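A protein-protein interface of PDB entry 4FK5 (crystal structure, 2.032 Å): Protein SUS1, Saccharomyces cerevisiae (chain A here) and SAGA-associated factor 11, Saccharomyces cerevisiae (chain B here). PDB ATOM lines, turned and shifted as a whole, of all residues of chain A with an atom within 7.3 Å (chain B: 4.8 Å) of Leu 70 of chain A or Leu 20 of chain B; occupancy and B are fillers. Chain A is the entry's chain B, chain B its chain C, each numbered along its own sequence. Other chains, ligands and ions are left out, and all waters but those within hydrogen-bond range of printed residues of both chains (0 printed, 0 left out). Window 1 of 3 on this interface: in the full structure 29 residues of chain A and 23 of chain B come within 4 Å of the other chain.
Of chain B, only Asn 17, Leu 20 and Ile 24 come within 4 Å of Leu 70 of chain A. Of the printed residues of chain A, Leu 20 of chain B touches Leu 33 (3.9 Å), Leu 70 (3.7 Å) and Arg 78 (3.8 Å). Of the printed residues of chain A, Leu 23 of chain B touches Leu 33 (3.6 Å) and Trp 38 (3.5 Å). Of the printed residues of chain A, Leu 16 of chain B touches Arg 78 (3.9 Å). Of the printed residues of chain B, Arg 78 of chain A touches Leu 16 (3.9 Å) and Leu 20 (3.8 Å). Of the printed residues of chain A, Asn 17 of chain B touches Leu 70 (3.97 Å). Of the printed residues of chain B, Leu 33 of chain A touches Leu 20 and Leu 23. Thr 77 of chain A touches none of the printed residues of chain B. The nearest residue of chain B that does not touch Leu 70 of chain A is Thr 21 of chain B (4.3 Å). The nearest printed residue of chain A that does not touch Leu 20 of chain B is Leu 29 of chain A (4.003 Å). The nearest printed residue of chain B that does not touch Leu 33 of chain A is Leu 19 of chain B (6.7 Å).
Hydrophobic or aromatic side chains of chain A that line the printed part of chain B: Leu 29, Leu 33, Trp 38, Ala 69 and Leu 70. Among the printed residues, 12 pairs touch across the chains. Among the printed residues, no Asp or Glu carboxylate lies within 4 Å of a Lys or Arg side-chain nitrogen of the other chain.
Among the printed residues, merely in contact across the chains: Leu 29 of chain A with Leu 19 of chain B (3.8 Å), Leu 33 of chain A with Leu 20 of chain B (3.9 Å), Leu 33 of chain A with Leu 23 of chain B (3.6 Å), Trp 38 of chain A with Leu 23 of chain B (3.5 Å), Trp 38 of chain A with Ile 24 of chain B (3.6 Å), Glu 66 of chain A with Thr 21 of chain B (3.6 Å), Ala 69 of chain A with Ile 24 of chain B (3.7 Å), Leu 70 of chain A with Asn 17 of chain B (3.97 Å), Leu 70 of chain A with Leu 20 of chain B (3.7 Å), Leu 70 of chain A with Ile 24 of chain B (3.8 Å), Arg 78 of chain A with Leu 16 of chain B (3.9 Å) and Arg 78 of chain A with Leu 20 of chain B (3.8 Å).
N of Trp 38 of chain A sits at hydrogen-bond distance from O of Leu 33 of chain A (3.0 Å). The indole nitrogen (NE1) of Trp 38 of chain A is in hydrogen-bond range of the backbone carbonyl oxygen (O) of Ala 69 of chain A, 3.0 Å away. O of Leu 70 of chain A lies within hydrogen-bond range of NH2 of Arg 78 of chain A. The backbone carbonyl oxygen (O) of Asn 17 of chain B sits at hydrogen-bond distance from the side-chain hydroxyl (OG1) of Thr 21 of chain B, at 2.9 Å. The side-chain hydroxyl (OG1) of Thr 21 of chain B lies within hydrogen-bond range of the backbone carbonyl oxygen (O) of Asn 18 of chain B, at 3.4 Å.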
ATOM      1  N   LEU A  29       7.410 -16.985 -10.687  1.00  0.00           N
ATOM      2  CA  LEU A  29       8.861 -17.058 -10.499  1.00  0.00           C
ATOM      3  C   LEU A  29       9.323 -18.454 -10.128  1.00  0.00           C
ATOM      4  O   LEU A  29      10.322 -18.933 -10.636  1.00  0.00           O
ATOM      5  CB  LEU A  29       9.293 -16.070  -9.421  1.00  0.00           C
ATOM      6  CG  LEU A  29      10.766 -16.131  -9.058  1.00  0.00           C
ATOM      7  CD1 LEU A  29      11.607 -15.650 -10.263  1.00  0.00           C
ATOM      8  CD2 LEU A  29      11.096 -15.282  -7.830  1.00  0.00           C
ATOM      9  N   LEU A  33      11.819 -20.858 -12.364  1.00  0.00           N
ATOM     10  CA  LEU A  33      13.087 -21.291 -11.789  1.00  0.00           C
ATOM     11  C   LEU A  33      13.181 -22.822 -11.720  1.00  0.00           C
ATOM     12  O   LEU A  33      14.245 -23.436 -11.952  1.00  0.00           O
ATOM     13  CB  LEU A  33      13.266 -20.692 -10.399  1.00  0.00           C
ATOM     14  CG  LEU A  33      13.440 -19.187 -10.319  1.00  0.00           C
ATOM     15  CD1 LEU A  33      13.559 -18.699  -8.835  1.00  0.00           C
ATOM     16  CD2 LEU A  33      14.664 -18.790 -11.143  1.00  0.00           C
ATOM     17  N   TRP A  38      17.102 -24.230 -12.124  1.00  0.00           N
ATOM     18  CA  TRP A  38      17.798 -23.420 -11.165  1.00  0.00           C
ATOM     19  C   TRP A  38      17.638 -23.934  -9.744  1.00  0.00           C
ATOM     20  O   TRP A  38      18.592 -23.899  -8.952  1.00  0.00           O
ATOM     21  CB  TRP A  38      17.304 -21.988 -11.266  1.00  0.00           C
ATOM     22  CG  TRP A  38      17.859 -21.054 -10.226  1.00  0.00           C
ATOM     23  CD1 TRP A  38      18.909 -20.172 -10.372  1.00  0.00           C
ATOM     24  CD2 TRP A  38      17.346 -20.811  -8.874  1.00  0.00           C
ATOM     25  NE1 TRP A  38      19.031 -19.374  -9.251  1.00  0.00           N
ATOM     26  CE2 TRP A  38      18.137 -19.726  -8.321  1.00  0.00           C
ATOM     27  CE3 TRP A  38      16.317 -21.336  -8.121  1.00  0.00           C
ATOM     28  CZ2 TRP A  38      17.924 -19.234  -7.057  1.00  0.00           C
ATOM     29  CZ3 TRP A  38      16.076 -20.805  -6.847  1.00  0.00           C
ATOM     30  CH2 TRP A  38      16.864 -19.787  -6.331  1.00  0.00           C
ATOM     31  N   VAL A  42      20.816 -24.924  -7.412  1.00  0.00           N
ATOM     32  CA  VAL A  42      21.116 -24.305  -6.122  1.00  0.00           C
ATOM     33  C   VAL A  42      21.340 -25.383  -5.049  1.00  0.00           C
ATOM     34  O   VAL A  42      22.241 -25.256  -4.205  1.00  0.00           O
ATOM     35  CB  VAL A  42      20.044 -23.304  -5.688  1.00  0.00           C
ATOM     36  CG1 VAL A  42      20.278 -22.835  -4.257  1.00  0.00           C
ATOM     37  CG2 VAL A  42      20.009 -22.152  -6.667  1.00  0.00           C
ATOM     38  N   LEU A  45      24.910 -26.704  -5.767  1.00  0.00           N
ATOM     39  CA  LEU A  45      25.854 -25.724  -5.323  1.00  0.00           C
ATOM     40  C   LEU A  45      25.973 -25.803  -3.806  1.00  0.00           C
ATOM     41  O   LEU A  45      27.052 -25.725  -3.264  1.00  0.00           O
ATOM     42  CB  LEU A  45      25.432 -24.320  -5.793  1.00  0.00           C
ATOM     43  CG  LEU A  45      26.126 -23.079  -5.192  1.00  0.00           C
ATOM     44  CD1 LEU A  45      27.650 -23.148  -5.416  1.00  0.00           C
ATOM     45  CD2 LEU A  45      25.521 -21.773  -5.778  1.00  0.00           C
ATOM     46  N   VAL A  65      26.790 -19.455  -0.860  1.00  0.00           N
ATOM     47  CA  VAL A  65      25.823 -19.878  -1.879  1.00  0.00           C
ATOM     48  C   VAL A  65      25.001 -18.698  -2.469  1.00  0.00           C
ATOM     49  O   VAL A  65      24.859 -18.581  -3.691  1.00  0.00           O
ATOM     50  CB  VAL A  65      24.895 -20.925  -1.315  1.00  0.00           C
ATOM     51  CG1 VAL A  65      23.742 -21.174  -2.286  1.00  0.00           C
ATOM     52  CG2 VAL A  65      25.700 -22.203  -1.018  1.00  0.00           C
ATOM     53  N   GLU A  66      24.454 -17.833  -1.597  1.00  0.00           N
ATOM     54  CA  GLU A  66      23.435 -16.855  -2.024  1.00  0.00           C
ATOM     55  C   GLU A  66      23.904 -15.956  -3.138  1.00  0.00           C
ATOM     56  O   GLU A  66      23.237 -15.871  -4.159  1.00  0.00           O
ATOM     57  CB  GLU A  66      22.923 -16.044  -0.848  1.00  0.00           C
ATOM     58  CG  GLU A  66      21.743 -15.161  -1.166  1.00  0.00           C
ATOM     59  CD  GLU A  66      21.105 -14.619   0.079  1.00  0.00           C
ATOM     60  OE1 GLU A  66      21.592 -13.595   0.556  1.00  0.00           O
ATOM     61  OE2 GLU A  66      20.144 -15.248   0.620  1.00  0.00           O
ATOM     62  N   PRO A  67      25.123 -15.355  -3.011  1.00  0.00           N
ATOM     63  CA  PRO A  67      25.585 -14.520  -4.121  1.00  0.00           C
ATOM     64  C   PRO A  67      25.612 -15.268  -5.453  1.00  0.00           C
ATOM     65  O   PRO A  67      25.170 -14.734  -6.475  1.00  0.00           O
ATOM     66  CB  PRO A  67      27.011 -14.104  -3.690  1.00  0.00           C
ATOM     67  CG  PRO A  67      27.006 -14.228  -2.215  1.00  0.00           C
ATOM     68  CD  PRO A  67      26.079 -15.367  -1.895  1.00  0.00           C
ATOM     69  N   LYS A  68      26.087 -16.495  -5.435  1.00  0.00           N
ATOM     70  CA  LYS A  68      26.217 -17.276  -6.675  1.00  0.00           C
ATOM     71  C   LYS A  68      24.829 -17.680  -7.246  1.00  0.00           C
ATOM     72  O   LYS A  68      24.598 -17.641  -8.449  1.00  0.00           O
ATOM     73  CB  LYS A  68      27.047 -18.526  -6.413  1.00  0.00           C
ATOM     74  CG  LYS A  68      28.549 -18.247  -6.309  1.00  0.00           C
ATOM     75  CD  LYS A  68      29.305 -19.449  -5.713  1.00  0.00           C
ATOM     76  CE  LYS A  68      30.791 -19.102  -5.456  1.00  0.00           C
ATOM     77  NZ  LYS A  68      31.542 -20.215  -4.796  1.00  0.00           N
ATOM     78  N   ALA A  69      23.922 -18.030  -6.356  1.00  0.00           N
ATOM     79  CA  ALA A  69      22.575 -18.448  -6.747  1.00  0.00           C
ATOM     80  C   ALA A  69      21.799 -17.266  -7.348  1.00  0.00           C
ATOM     81  O   ALA A  69      21.109 -17.435  -8.299  1.00  0.00           O
ATOM     82  CB  ALA A  69      21.829 -19.045  -5.533  1.00  0.00           C
ATOM     83  N   LEU A  70      21.961 -16.071  -6.791  1.00  0.00           N
ATOM     84  CA  LEU A  70      21.403 -14.854  -7.408  1.00  0.00           C
ATOM     85  C   LEU A  70      21.858 -14.681  -8.841  1.00  0.00           C
ATOM     86  O   LEU A  70      21.049 -14.375  -9.708  1.00  0.00           O
ATOM     87  CB  LEU A  70      21.723 -13.581  -6.586  1.00  0.00           C
ATOM     88  CG  LEU A  70      21.006 -13.416  -5.234  1.00  0.00           C
ATOM     89  CD1 LEU A  70      21.545 -12.192  -4.510  1.00  0.00           C
ATOM     90  CD2 LEU A  70      19.465 -13.331  -5.382  1.00  0.00           C
ATOM     91  N   GLU A  71      23.160 -14.894  -9.103  1.00  0.00           N
ATOM     92  CA  GLU A  71      23.727 -14.710 -10.463  1.00  0.00           C
ATOM     93  C   GLU A  71      23.317 -15.851 -11.412  1.00  0.00           C
ATOM     94  O   GLU A  71      23.362 -15.695 -12.601  1.00  0.00           O
ATOM     95  CB  GLU A  71      25.282 -14.613 -10.418  1.00  0.00           C
ATOM     96  CG  GLU A  71      25.809 -13.489  -9.529  1.00  0.00           C
ATOM     97  CD  GLU A  71      27.340 -13.428  -9.477  1.00  0.00           C
ATOM     98  OE1 GLU A  71      27.932 -13.831  -8.437  1.00  0.00           O
ATOM     99  OE2 GLU A  71      27.951 -12.980 -10.477  1.00  0.00           O
ATOM    100  N   MET A  72      22.930 -16.992 -10.872  1.00  0.00           N
ATOM    101  CA  MET A  72      22.584 -18.122 -11.728  1.00  0.00           C
ATOM    102  C   MET A  72      21.178 -17.987 -12.333  1.00  0.00           C
ATOM    103  O   MET A  72      20.828 -18.756 -13.188  1.00  0.00           O
ATOM    104  CB  MET A  72      22.652 -19.424 -10.968  1.00  0.00           C
ATOM    105  CG  MET A  72      24.059 -19.911 -10.626  1.00  0.00           C
ATOM    106  SD  MET A  72      23.959 -21.191  -9.364  1.00  0.00           S
ATOM    107  CE  MET A  72      23.460 -22.581 -10.341  1.00  0.00           C
ATOM    108  N   VAL A  73      20.353 -17.060 -11.818  1.00  0.00           N
ATOM    109  CA  VAL A  73      19.033 -16.828 -12.393  1.00  0.00           C
ATOM    110  C   VAL A  73      19.213 -16.408 -13.864  1.00  0.00           C
ATOM    111  O   VAL A  73      19.975 -15.500 -14.163  1.00  0.00           O
ATOM    112  CB  VAL A  73      18.236 -15.723 -11.609  1.00  0.00           C
ATOM    113  CG1 VAL A  73      16.888 -15.488 -12.246  1.00  0.00           C
ATOM    114  CG2 VAL A  73      18.052 -16.105 -10.133  1.00  0.00           C
ATOM    115  N   SER A  74      18.517 -17.076 -14.767  1.00  0.00           N
ATOM    116  CA  SER A  74      18.617 -16.749 -16.162  1.00  0.00           C
ATOM    117  C   SER A  74      18.166 -15.332 -16.456  1.00  0.00           C
ATOM    118  O   SER A  74      17.278 -14.772 -15.761  1.00  0.00           O
ATOM    119  CB  SER A  74      17.811 -17.725 -17.000  1.00  0.00           C
ATOM    120  OG  SER A  74      16.435 -17.432 -16.917  1.00  0.00           O
ATOM    121  N   THR A  77      14.236 -15.254 -17.148  1.00  0.00           N
ATOM    122  CA  THR A  77      13.430 -15.293 -15.937  1.00  0.00           C
ATOM    123  C   THR A  77      13.521 -13.981 -15.211  1.00  0.00           C
ATOM    124  O   THR A  77      12.479 -13.385 -14.835  1.00  0.00           O
ATOM    125  CB  THR A  77      13.853 -16.457 -15.012  1.00  0.00           C
ATOM    126  OG1 THR A  77      13.477 -17.678 -15.625  1.00  0.00           O
ATOM    127  CG2 THR A  77      13.223 -16.341 -13.677  1.00  0.00           C
ATOM    128  N   ARG A  78      14.739 -13.479 -15.035  1.00  0.00           N
ATOM    129  CA  ARG A  78      14.919 -12.253 -14.272  1.00  0.00           C
ATOM    130  C   ARG A  78      14.184 -11.075 -14.953  1.00  0.00           C
ATOM    131  O   ARG A  78      13.409 -10.352 -14.279  1.00  0.00           O
ATOM    132  CB  ARG A  78      16.405 -11.904 -14.049  1.00  0.00           C
ATOM    133  CG  ARG A  78      16.605 -10.604 -13.265  1.00  0.00           C
ATOM    134  CD  ARG A  78      18.083 -10.242 -13.108  1.00  0.00           C
ATOM    135  NE  ARG A  78      18.713 -11.098 -12.111  1.00  0.00           N
ATOM    136  CZ  ARG A  78      18.630 -10.915 -10.799  1.00  0.00           C
ATOM    137  NH1 ARG A  78      17.986  -9.839 -10.298  1.00  0.00           N
ATOM    138  NH2 ARG A  78      19.186 -11.808  -9.976  1.00  0.00           N
ATOM    139  N   LEU B  16      11.880  -8.400  -6.229  1.00  0.00           N
ATOM    140  CA  LEU B  16      12.449  -9.602  -6.756  1.00  0.00           C
ATOM    141  C   LEU B  16      13.510 -10.137  -5.848  1.00  0.00           C
ATOM    142  O   LEU B  16      13.561 -11.345  -5.603  1.00  0.00           O
ATOM    143  CB  LEU B  16      13.026  -9.381  -8.174  1.00  0.00           C
ATOM    144  CG  LEU B  16      13.581 -10.613  -8.869  1.00  0.00           C
ATOM    145  CD1 LEU B  16      12.565 -11.727  -8.932  1.00  0.00           C
ATOM    146  CD2 LEU B  16      14.095 -10.262 -10.251  1.00  0.00           C
ATOM    147  N   ASN B  17      14.351  -9.239  -5.305  1.00  0.00           N
ATOM    148  CA  ASN B  17      15.391  -9.672  -4.408  1.00  0.00           C
ATOM    149  C   ASN B  17      14.815 -10.278  -3.114  1.00  0.00           C
ATOM    150  O   ASN B  17      15.338 -11.266  -2.608  1.00  0.00           O
ATOM    151  CB  ASN B  17      16.360  -8.546  -4.087  1.00  0.00           C
ATOM    152  CG  ASN B  17      17.575  -9.019  -3.255  1.00  0.00           C
ATOM    153  OD1 ASN B  17      17.651  -8.738  -2.060  1.00  0.00           O
ATOM    154  ND2 ASN B  17      18.500  -9.720  -3.876  1.00  0.00           N
ATOM    155  N   ASN B  18      13.726  -9.716  -2.610  1.00  0.00           N
ATOM    156  CA  ASN B  18      13.012 -10.383  -1.506  1.00  0.00           C
ATOM    157  C   ASN B  18      12.597 -11.804  -1.890  1.00  0.00           C
ATOM    158  O   ASN B  18      12.954 -12.766  -1.230  1.00  0.00           O
ATOM    159  CB  ASN B  18      11.840  -9.516  -0.975  1.00  0.00           C
ATOM    160  CG  ASN B  18      12.312  -8.407   0.032  1.00  0.00           C
ATOM    161  OD1 ASN B  18      11.547  -7.971   0.941  1.00  0.00           O
ATOM    162  ND2 ASN B  18      13.473  -7.919  -0.169  1.00  0.00           N
ATOM    163  N   LEU B  19      11.920 -11.955  -3.015  1.00  0.00           N
ATOM    164  CA  LEU B  19      11.477 -13.280  -3.416  1.00  0.00           C
ATOM    165  C   LEU B  19      12.641 -14.241  -3.592  1.00  0.00           C
ATOM    166  O   LEU B  19      12.570 -15.375  -3.125  1.00  0.00           O
ATOM    167  CB  LEU B  19      10.677 -13.214  -4.680  1.00  0.00           C
ATOM    168  CG  LEU B  19       9.326 -12.512  -4.573  1.00  0.00           C
ATOM    169  CD1 LEU B  19       8.880 -12.043  -5.956  1.00  0.00           C
ATOM    170  CD2 LEU B  19       8.275 -13.456  -3.956  1.00  0.00           C
ATOM    171  N   LEU B  20      13.707 -13.810  -4.288  1.00  0.00           N
ATOM    172  CA  LEU B  20      14.818 -14.683  -4.572  1.00  0.00           C
ATOM    173  C   LEU B  20      15.623 -15.095  -3.315  1.00  0.00           C
ATOM    174  O   LEU B  20      15.879 -16.266  -3.137  1.00  0.00           O
ATOM    175  CB  LEU B  20      15.796 -14.048  -5.588  1.00  0.00           C
ATOM    176  CG  LEU B  20      15.263 -14.011  -7.036  1.00  0.00           C
ATOM    177  CD1 LEU B  20      16.273 -13.155  -7.929  1.00  0.00           C
ATOM    178  CD2 LEU B  20      15.084 -15.414  -7.515  1.00  0.00           C
ATOM    179  N   THR B  21      16.008 -14.132  -2.476  1.00  0.00           N
ATOM    180  CA  THR B  21      16.815 -14.478  -1.264  1.00  0.00           C
ATOM    181  C   THR B  21      16.009 -15.386  -0.322  1.00  0.00           C
ATOM    182  O   THR B  21      16.551 -16.328   0.228  1.00  0.00           O
ATOM    183  CB  THR B  21      17.297 -13.255  -0.459  1.00  0.00           C
ATOM    184  OG1 THR B  21      16.184 -12.475  -0.077  1.00  0.00           O
ATOM    185  CG2 THR B  21      18.348 -12.321  -1.312  1.00  0.00           C
ATOM    186  N   THR B  22      14.704 -15.135  -0.205  1.00  0.00           N
ATOM    187  CA  THR B  22      13.846 -16.044   0.552  1.00  0.00           C
ATOM    188  C   THR B  22      13.901 -17.441   0.068  1.00  0.00           C
ATOM    189  O   THR B  22      14.070 -18.388   0.866  1.00  0.00           O
ATOM    190  CB  THR B  22      12.375 -15.532   0.648  1.00  0.00           C
ATOM    191  OG1 THR B  22      12.375 -14.254   1.250  1.00  0.00           O
ATOM    192  CG2 THR B  22      11.513 -16.506   1.499  1.00  0.00           C
ATOM    193  N   LEU B  23      13.750 -17.625  -1.225  1.00  0.00           N
ATOM    194  CA  LEU B  23      13.743 -18.960  -1.811  1.00  0.00           C
ATOM    195  C   LEU B  23      15.105 -19.663  -1.716  1.00  0.00           C
ATOM    196  O   LEU B  23      15.180 -20.846  -1.386  1.00  0.00           O
ATOM    197  CB  LEU B  23      13.312 -18.865  -3.269  1.00  0.00           C
ATOM    198  CG  LEU B  23      13.267 -20.176  -4.051  1.00  0.00           C
ATOM    199  CD1 LEU B  23      12.253 -21.197  -3.417  1.00  0.00           C
ATOM    200  CD2 LEU B  23      12.918 -19.901  -5.524  1.00  0.00           C
ATOM    201  N   ILE B  24      16.183 -18.909  -1.923  1.00  0.00           N
ATOM    202  CA  ILE B  24      17.531 -19.448  -1.705  1.00  0.00           C
ATOM    203  C   ILE B  24      17.743 -19.828  -0.237  1.00  0.00           C
ATOM    204  O   ILE B  24      18.229 -20.851   0.042  1.00  0.00           O
ATOM    205  CB  ILE B  24      18.620 -18.439  -2.077  1.00  0.00           C
ATOM    206  CG1 ILE B  24      18.642 -18.185  -3.600  1.00  0.00           C
ATOM    207  CG2 ILE B  24      20.000 -18.959  -1.622  1.00  0.00           C
ATOM    208  CD1 ILE B  24      19.276 -16.832  -3.966  1.00  0.00           C
